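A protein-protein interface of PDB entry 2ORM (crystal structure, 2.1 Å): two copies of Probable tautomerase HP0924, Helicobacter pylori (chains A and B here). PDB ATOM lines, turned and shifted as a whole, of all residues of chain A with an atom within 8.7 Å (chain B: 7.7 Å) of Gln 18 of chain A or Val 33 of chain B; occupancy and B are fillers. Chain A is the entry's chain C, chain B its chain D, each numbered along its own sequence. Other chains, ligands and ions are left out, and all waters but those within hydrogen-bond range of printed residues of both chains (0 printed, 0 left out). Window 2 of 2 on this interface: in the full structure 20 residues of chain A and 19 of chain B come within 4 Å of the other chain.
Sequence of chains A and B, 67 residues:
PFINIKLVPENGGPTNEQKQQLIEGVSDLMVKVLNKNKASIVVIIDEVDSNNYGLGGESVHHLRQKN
The side-chain amide nitrogen (NE2) of Gln 18 of chain A is in hydrogen-bond range of the backbone carbonyl oxygen (O) of Val 33 of chain B, 3.3 Å away.
The side-chain amide oxygen (OE1) of Gln 18 of chain A is in hydrogen-bond range of the backbone NH (N) of Thr 15 of chain A (3.0 Å).
CD2 of Leu 7 of chain A touches CD1 of Leu 34 of chain B, at 3.9 Å.
CD2 of Leu 34 of chain B touches CB of Pro 14 of chain A, 3.8 Å away.
CD2 of Leu 34 of chain B touches NE2 of Gln 18 of chain A, 3.7 Å away.
Val 33 of chain B touches Gln 21 of chain A (CG1 to OE1, 3.8 Å).
Gly 25 of chain A touches Leu 29 of chain B (C to CD2, 3.9 Å).
Leu 29 of chain B touches Val 26 of chain A (CD2 to CG1, 3.4 Å).
Gly 12 of chain A touches none of the printed residues of chain B.
Gln 18 of chain A touches just these residues of chain B: Val 33 (3.3 Å) and Leu 34 (3.7 Å).
Printed residues of chain B within 4 Å of Gln 21 of chain A: Val 33 (3.8 Å).
Asp 28 of chain B touches none of the printed residues of chain A.
No residue of chain A comes within 4 Å of Lys 32 of chain B.
Printed residues of chain A within 4 Å of Val 33 of chain B: Gln 18 and Gln 21.
Of the printed residues of chain A, Leu 34 of chain B touches Leu 7 (3.9 Å), Pro 14 (3.8 Å) and Gln 18 (3.7 Å).
The nearest printed residue of chain B that does not touch Gln 21 of chain A is Leu 29 of chain B (4.8 Å).
Printed residues of chain B that touch a printed residue of chain A: Leu 29, Val 33 and Leu 34.
Hydrophobic or aromatic side chains of chain B within 4 Å of the printed part of chain A: Leu 29, Val 33 and Leu 34.
Hydrophobic or aromatic side chains of chain A that line the printed part of chain B: Leu 7, Pro 14 and Val 26.
Among the printed residues, 7 pairs touch across the chains.
Among the printed residues, no Asp or Glu carboxylate lies within 4 Å of a Lys or Arg side-chain nitrogen of the other chain.
No position is printed for both chains.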
ATOM      1  N   ILE A   5      11.891 -16.672  17.737  1.00  0.00           N
ATOM      2  CA  ILE A   5      12.182 -18.061  17.401  1.00  0.00           C
ATOM      3  C   ILE A   5      13.343 -18.547  18.279  1.00  0.00           C
ATOM      4  O   ILE A   5      14.399 -17.920  18.313  1.00  0.00           O
ATOM      5  CB  ILE A   5      12.593 -18.201  15.898  1.00  0.00           C
ATOM      6  CG1 ILE A   5      11.457 -17.723  14.987  1.00  0.00           C
ATOM      7  CG2 ILE A   5      12.947 -19.643  15.584  1.00  0.00           C
ATOM      8  CD1 ILE A   5      11.845 -17.621  13.510  1.00  0.00           C
ATOM      9  N   LEU A   7      15.668 -21.887  18.940  1.00  0.00           N
ATOM     10  CA  LEU A   7      16.052 -23.161  18.356  1.00  0.00           C
ATOM     11  C   LEU A   7      17.407 -23.653  18.863  1.00  0.00           C
ATOM     12  O   LEU A   7      18.232 -22.872  19.355  1.00  0.00           O
ATOM     13  CB  LEU A   7      16.083 -23.023  16.828  1.00  0.00           C
ATOM     14  CG  LEU A   7      16.886 -21.839  16.268  1.00  0.00           C
ATOM     15  CD1 LEU A   7      18.363 -22.193  16.204  1.00  0.00           C
ATOM     16  CD2 LEU A   7      16.382 -21.494  14.872  1.00  0.00           C
ATOM     17  N   GLU A  10      22.317 -27.102  15.350  1.00  0.00           N
ATOM     18  CA  GLU A  10      22.613 -28.485  15.013  1.00  0.00           C
ATOM     19  C   GLU A  10      23.530 -28.601  13.804  1.00  0.00           C
ATOM     20  O   GLU A  10      23.386 -27.865  12.822  1.00  0.00           O
ATOM     21  CB  GLU A  10      21.318 -29.251  14.762  1.00  0.00           C
ATOM     22  N   ASN A  11      24.470 -29.537  13.897  1.00  0.00           N
ATOM     23  CA  ASN A  11      25.437 -29.825  12.841  1.00  0.00           C
ATOM     24  C   ASN A  11      25.878 -28.620  12.017  1.00  0.00           C
ATOM     25  O   ASN A  11      25.566 -28.525  10.828  1.00  0.00           O
ATOM     26  CB  ASN A  11      24.883 -30.919  11.917  1.00  0.00           C
ATOM     27  N   GLY A  12      26.604 -27.707  12.653  1.00  0.00           N
ATOM     28  CA  GLY A  12      27.101 -26.532  11.959  1.00  0.00           C
ATOM     29  C   GLY A  12      26.057 -25.585  11.398  1.00  0.00           C
ATOM     30  O   GLY A  12      26.253 -24.995  10.331  1.00  0.00           O
ATOM     31  N   GLY A  13      24.950 -25.425  12.117  1.00  0.00           N
ATOM     32  CA  GLY A  13      23.899 -24.532  11.663  1.00  0.00           C
ATOM     33  C   GLY A  13      23.165 -23.940  12.850  1.00  0.00           C
ATOM     34  O   GLY A  13      23.306 -24.445  13.966  1.00  0.00           O
ATOM     35  N   PRO A  14      22.372 -22.874  12.650  1.00  0.00           N
ATOM     36  CA  PRO A  14      22.132 -22.200  11.369  1.00  0.00           C
ATOM     37  C   PRO A  14      23.188 -21.160  10.995  1.00  0.00           C
ATOM     38  O   PRO A  14      23.800 -20.537  11.867  1.00  0.00           O
ATOM     39  CB  PRO A  14      20.765 -21.564  11.580  1.00  0.00           C
ATOM     40  CG  PRO A  14      20.836 -21.160  13.018  1.00  0.00           C
ATOM     41  CD  PRO A  14      21.437 -22.378  13.678  1.00  0.00           C
ATOM     42  N   THR A  15      23.395 -20.978   9.694  1.00  0.00           N
ATOM     43  CA  THR A  15      24.356 -19.998   9.191  1.00  0.00           C
ATOM     44  C   THR A  15      23.659 -18.638   9.111  1.00  0.00           C
ATOM     45  O   THR A  15      22.431 -18.565   9.191  1.00  0.00           O
ATOM     46  CB  THR A  15      24.838 -20.363   7.771  1.00  0.00           C
ATOM     47  OG1 THR A  15      23.729 -20.319   6.870  1.00  0.00           O
ATOM     48  CG2 THR A  15      25.438 -21.764   7.744  1.00  0.00           C
ATOM     49  N   ASN A  16      24.431 -17.567   8.943  1.00  0.00           N
ATOM     50  CA  ASN A  16      23.841 -16.237   8.832  1.00  0.00           C
ATOM     51  C   ASN A  16      22.897 -16.181   7.626  1.00  0.00           C
ATOM     52  O   ASN A  16      21.927 -15.421   7.623  1.00  0.00           O
ATOM     53  CB  ASN A  16      24.930 -15.162   8.704  1.00  0.00           C
ATOM     54  CG  ASN A  16      25.704 -14.964   9.993  1.00  0.00           C
ATOM     55  OD1 ASN A  16      25.334 -15.495  11.041  1.00  0.00           O
ATOM     56  ND2 ASN A  16      26.782 -14.187   9.926  1.00  0.00           N
ATOM     57  N   GLU A  17      23.164 -17.004   6.614  1.00  0.00           N
ATOM     58  CA  GLU A  17      22.321 -17.042   5.420  1.00  0.00           C
ATOM     59  C   GLU A  17      20.960 -17.670   5.709  1.00  0.00           C
ATOM     60  O   GLU A  17      19.937 -17.187   5.228  1.00  0.00           O
ATOM     61  CB  GLU A  17      23.008 -17.823   4.292  1.00  0.00           C
ATOM     62  CG  GLU A  17      24.291 -17.181   3.768  1.00  0.00           C
ATOM     63  CD  GLU A  17      25.463 -17.342   4.720  1.00  0.00           C
ATOM     64  OE1 GLU A  17      26.506 -16.689   4.497  1.00  0.00           O
ATOM     65  OE2 GLU A  17      25.346 -18.125   5.685  1.00  0.00           O
ATOM     66  N   GLN A  18      20.953 -18.753   6.485  1.00  0.00           N
ATOM     67  CA  GLN A  18      19.710 -19.433   6.845  1.00  0.00           C
ATOM     68  C   GLN A  18      18.876 -18.550   7.770  1.00  0.00           C
ATOM     69  O   GLN A  18      17.644 -18.589   7.737  1.00  0.00           O
ATOM     70  CB  GLN A  18      20.003 -20.757   7.555  1.00  0.00           C
ATOM     71  CG  GLN A  18      20.684 -21.785   6.687  1.00  0.00           C
ATOM     72  CD  GLN A  18      20.977 -23.066   7.434  1.00  0.00           C
ATOM     73  OE1 GLN A  18      21.750 -23.082   8.406  1.00  0.00           O
ATOM     74  NE2 GLN A  18      20.359 -24.154   6.990  1.00  0.00           N
ATOM     75  N   LYS A  19      19.554 -17.772   8.611  1.00  0.00           N
ATOM     76  CA  LYS A  19      18.856 -16.871   9.518  1.00  0.00           C
ATOM     77  C   LYS A  19      18.124 -15.829   8.678  1.00  0.00           C
ATOM     78  O   LYS A  19      16.974 -15.497   8.962  1.00  0.00           O
ATOM     79  CB  LYS A  19      19.847 -16.191  10.469  1.00  0.00           C
ATOM     80  CG  LYS A  19      20.447 -17.135  11.518  1.00  0.00           C
ATOM     81  CD  LYS A  19      21.496 -16.427  12.368  1.00  0.00           C
ATOM     82  CE  LYS A  19      22.047 -17.341  13.446  1.00  0.00           C
ATOM     83  NZ  LYS A  19      23.163 -16.708  14.204  1.00  0.00           N
ATOM     84  N   GLN A  20      18.791 -15.329   7.639  1.00  0.00           N
ATOM     85  CA  GLN A  20      18.195 -14.338   6.746  1.00  0.00           C
ATOM     86  C   GLN A  20      16.963 -14.906   6.050  1.00  0.00           C
ATOM     87  O   GLN A  20      15.955 -14.218   5.894  1.00  0.00           O
ATOM     88  CB  GLN A  20      19.207 -13.884   5.694  1.00  0.00           C
ATOM     89  CG  GLN A  20      18.646 -12.891   4.674  1.00  0.00           C
ATOM     90  CD  GLN A  20      18.167 -11.589   5.300  1.00  0.00           C
ATOM     91  OE1 GLN A  20      18.934 -10.882   5.957  1.00  0.00           O
ATOM     92  NE2 GLN A  20      16.895 -11.265   5.093  1.00  0.00           N
ATOM     93  N   GLN A  21      17.046 -16.164   5.625  1.00  0.00           N
ATOM     94  CA  GLN A  21      15.914 -16.803   4.961  1.00  0.00           C
ATOM     95  C   GLN A  21      14.708 -16.931   5.885  1.00  0.00           C
ATOM     96  O   GLN A  21      13.563 -16.745   5.459  1.00  0.00           O
ATOM     97  CB  GLN A  21      16.317 -18.184   4.449  1.00  0.00           C
ATOM     98  CG  GLN A  21      17.239 -18.154   3.241  1.00  0.00           C
ATOM     99  CD  GLN A  21      17.531 -19.541   2.715  1.00  0.00           C
ATOM    100  OE1 GLN A  21      18.174 -20.351   3.391  1.00  0.00           O
ATOM    101  NE2 GLN A  21      17.053 -19.829   1.508  1.00  0.00           N
ATOM    102  N   LEU A  22      14.970 -17.256   7.150  1.00  0.00           N
ATOM    103  CA  LEU A  22      13.915 -17.398   8.154  1.00  0.00           C
ATOM    104  C   LEU A  22      13.239 -16.060   8.388  1.00  0.00           C
ATOM    105  O   LEU A  22      12.013 -15.976   8.486  1.00  0.00           O
ATOM    106  CB  LEU A  22      14.500 -17.891   9.482  1.00  0.00           C
ATOM    107  CG  LEU A  22      14.922 -19.357   9.559  1.00  0.00           C
ATOM    108  CD1 LEU A  22      15.601 -19.615  10.884  1.00  0.00           C
ATOM    109  CD2 LEU A  22      13.691 -20.252   9.379  1.00  0.00           C
ATOM    110  N   ILE A  23      14.059 -15.019   8.491  1.00  0.00           N
ATOM    111  CA  ILE A  23      13.575 -13.662   8.708  1.00  0.00           C
ATOM    112  C   ILE A  23      12.668 -13.212   7.559  1.00  0.00           C
ATOM    113  O   ILE A  23      11.539 -12.783   7.780  1.00  0.00           O
ATOM    114  CB  ILE A  23      14.776 -12.696   8.871  1.00  0.00           C
ATOM    115  CG1 ILE A  23      15.452 -12.947  10.227  1.00  0.00           C
ATOM    116  CG2 ILE A  23      14.321 -11.241   8.730  1.00  0.00           C
ATOM    117  CD1 ILE A  23      16.716 -12.140  10.463  1.00  0.00           C
ATOM    118  N   GLU A  24      13.161 -13.338   6.331  1.00  0.00           N
ATOM    119  CA  GLU A  24      12.402 -12.951   5.142  1.00  0.00           C
ATOM    120  C   GLU A  24      11.147 -13.796   4.919  1.00  0.00           C
ATOM    121  O   GLU A  24      10.120 -13.283   4.477  1.00  0.00           O
ATOM    122  CB  GLU A  24      13.300 -13.035   3.910  1.00  0.00           C
ATOM    123  N   GLY A  25      11.242 -15.090   5.219  1.00  0.00           N
ATOM    124  CA  GLY A  25      10.119 -15.992   5.030  1.00  0.00           C
ATOM    125  C   GLY A  25       8.952 -15.765   5.970  1.00  0.00           C
ATOM    126  O   GLY A  25       7.802 -15.713   5.526  1.00  0.00           O
ATOM    127  N   VAL A  26       9.230 -15.649   7.271  1.00  0.00           N
ATOM    128  CA  VAL A  26       8.164 -15.409   8.238  1.00  0.00           C
ATOM    129  C   VAL A  26       7.571 -14.029   7.961  1.00  0.00           C
ATOM    130  O   VAL A  26       6.369 -13.822   8.109  1.00  0.00           O
ATOM    131  CB  VAL A  26       8.680 -15.457   9.715  1.00  0.00           C
ATOM    132  CG1 VAL A  26       9.189 -16.846  10.046  1.00  0.00           C
ATOM    133  CG2 VAL A  26       9.781 -14.443   9.922  1.00  0.00           C
ATOM    134  N   ILE A  45      15.853 -14.184  16.849  1.00  0.00           N
ATOM    135  CA  ILE A  45      16.221 -15.593  16.912  1.00  0.00           C
ATOM    136  C   ILE A  45      17.149 -15.897  18.089  1.00  0.00           C
ATOM    137  O   ILE A  45      18.214 -15.309  18.206  1.00  0.00           O
ATOM    138  CB  ILE A  45      16.916 -16.029  15.603  1.00  0.00           C
ATOM    139  CG1 ILE A  45      15.955 -15.844  14.425  1.00  0.00           C
ATOM    140  CG2 ILE A  45      17.379 -17.483  15.707  1.00  0.00           C
ATOM    141  CD1 ILE A  45      16.597 -16.064  13.065  1.00  0.00           C
ATOM    142  N   SER B  27       5.642 -23.608  10.189  1.00  0.00           N
ATOM    143  CA  SER B  27       6.147 -24.962  10.404  1.00  0.00           C
ATOM    144  C   SER B  27       6.842 -25.467   9.145  1.00  0.00           C
ATOM    145  O   SER B  27       7.999 -25.902   9.196  1.00  0.00           O
ATOM    146  CB  SER B  27       4.999 -25.897  10.788  1.00  0.00           C
ATOM    147  OG  SER B  27       4.375 -25.463  11.986  1.00  0.00           O
ATOM    148  N   ASP B  28       6.131 -25.397   8.019  1.00  0.00           N
ATOM    149  CA  ASP B  28       6.666 -25.811   6.726  1.00  0.00           C
ATOM    150  C   ASP B  28       7.940 -25.023   6.440  1.00  0.00           C
ATOM    151  O   ASP B  28       8.863 -25.523   5.797  1.00  0.00           O
ATOM    152  CB  ASP B  28       5.639 -25.545   5.616  1.00  0.00           C
ATOM    153  CG  ASP B  28       4.476 -26.531   5.637  1.00  0.00           C
ATOM    154  OD1 ASP B  28       3.495 -26.300   4.898  1.00  0.00           O
ATOM    155  OD2 ASP B  28       4.543 -27.537   6.384  1.00  0.00           O
ATOM    156  N   LEU B  29       7.988 -23.785   6.921  1.00  0.00           N
ATOM    157  CA  LEU B  29       9.162 -22.945   6.717  1.00  0.00           C
ATOM    158  C   LEU B  29      10.372 -23.499   7.463  1.00  0.00           C
ATOM    159  O   LEU B  29      11.479 -23.547   6.915  1.00  0.00           O
ATOM    160  CB  LEU B  29       8.887 -21.512   7.186  1.00  0.00           C
ATOM    161  CG  LEU B  29      10.057 -20.529   7.043  1.00  0.00           C
ATOM    162  CD1 LEU B  29      10.438 -20.394   5.574  1.00  0.00           C
ATOM    163  CD2 LEU B  29       9.668 -19.178   7.617  1.00  0.00           C
ATOM    164  N   MET B  30      10.168 -23.911   8.711  1.00  0.00           N
ATOM    165  CA  MET B  30      11.266 -24.457   9.503  1.00  0.00           C
ATOM    166  C   MET B  30      11.809 -25.703   8.814  1.00  0.00           C
ATOM    167  O   MET B  30      13.010 -25.956   8.826  1.00  0.00           O
ATOM    168  CB  MET B  30      10.792 -24.821  10.914  1.00  0.00           C
ATOM    169  CG  MET B  30      10.237 -23.649  11.728  1.00  0.00           C
ATOM    170  SD  MET B  30      11.472 -22.382  12.052  1.00  0.00           S
ATOM    171  CE  MET B  30      12.257 -23.017  13.515  1.00  0.00           C
ATOM    172  N   VAL B  31      10.911 -26.478   8.210  1.00  0.00           N
ATOM    173  CA  VAL B  31      11.299 -27.696   7.512  1.00  0.00           C
ATOM    174  C   VAL B  31      12.096 -27.365   6.255  1.00  0.00           C
ATOM    175  O   VAL B  31      13.168 -27.923   6.024  1.00  0.00           O
ATOM    176  CB  VAL B  31      10.059 -28.526   7.100  1.00  0.00           C
ATOM    177  CG1 VAL B  31      10.489 -29.749   6.304  1.00  0.00           C
ATOM    178  CG2 VAL B  31       9.282 -28.952   8.339  1.00  0.00           C
ATOM    179  N   LYS B  32      11.573 -26.448   5.447  1.00  0.00           N
ATOM    180  CA  LYS B  32      12.230 -26.062   4.205  1.00  0.00           C
ATOM    181  C   LYS B  32      13.617 -25.458   4.404  1.00  0.00           C
ATOM    182  O   LYS B  32      14.552 -25.790   3.681  1.00  0.00           O
ATOM    183  CB  LYS B  32      11.354 -25.093   3.435  1.00  0.00           C
ATOM    184  N   VAL B  33      13.760 -24.578   5.387  1.00  0.00           N
ATOM    185  CA  VAL B  33      15.045 -23.936   5.617  1.00  0.00           C
ATOM    186  C   VAL B  33      16.034 -24.693   6.503  1.00  0.00           C
ATOM    187  O   VAL B  33      17.229 -24.720   6.210  1.00  0.00           O
ATOM    188  CB  VAL B  33      14.854 -22.522   6.211  1.00  0.00           C
ATOM    189  CG1 VAL B  33      16.189 -21.805   6.284  1.00  0.00           C
ATOM    190  CG2 VAL B  33      13.875 -21.729   5.360  1.00  0.00           C
ATOM    191  N   LEU B  34      15.547 -25.316   7.573  1.00  0.00           N
ATOM    192  CA  LEU B  34      16.435 -26.023   8.496  1.00  0.00           C
ATOM    193  C   LEU B  34      16.289 -27.538   8.531  1.00  0.00           C
ATOM    194  O   LEU B  34      17.049 -28.219   9.217  1.00  0.00           O
ATOM    195  CB  LEU B  34      16.251 -25.479   9.915  1.00  0.00           C
ATOM    196  CG  LEU B  34      16.622 -24.018  10.179  1.00  0.00           C
ATOM    197  CD1 LEU B  34      16.236 -23.653  11.604  1.00  0.00           C
ATOM    198  CD2 LEU B  34      18.116 -23.809   9.958  1.00  0.00           C
ATOM    199  N   ASN B  35      15.318 -28.065   7.798  1.00  0.00           N
ATOM    200  CA  ASN B  35      15.084 -29.500   7.771  1.00  0.00           C
ATOM    201  C   ASN B  35      14.786 -30.020   9.181  1.00  0.00           C
ATOM    202  O   ASN B  35      15.197 -31.120   9.551  1.00  0.00           O
ATOM    203  CB  ASN B  35      16.303 -30.227   7.199  1.00  0.00           C
ATOM    204  CG  ASN B  35      15.958 -31.601   6.653  1.00  0.00           C
ATOM    205  OD1 ASN B  35      15.442 -32.459   7.370  1.00  0.00           O
ATOM    206  ND2 ASN B  35      16.238 -31.814   5.373  1.00  0.00           N
ATOM    207  N   LYS B  36      14.081 -29.214   9.970  1.00  0.00           N
ATOM    208  CA  LYS B  36      13.707 -29.602  11.323  1.00  0.00           C
ATOM    209  C   LYS B  36      12.531 -30.575  11.256  1.00  0.00           C
ATOM    210  O   LYS B  36      11.863 -30.676  10.225  1.00  0.00           O
ATOM    211  CB  LYS B  36      13.289 -28.371  12.131  1.00  0.00           C
ATOM    212  CG  LYS B  36      14.426 -27.440  12.509  1.00  0.00           C
ATOM    213  CD  LYS B  36      15.348 -28.102  13.517  1.00  0.00           C
ATOM    214  CE  LYS B  36      16.349 -27.110  14.074  1.00  0.00           C
ATOM    215  NZ  LYS B  36      17.271 -27.764  15.028  1.00  0.00           N
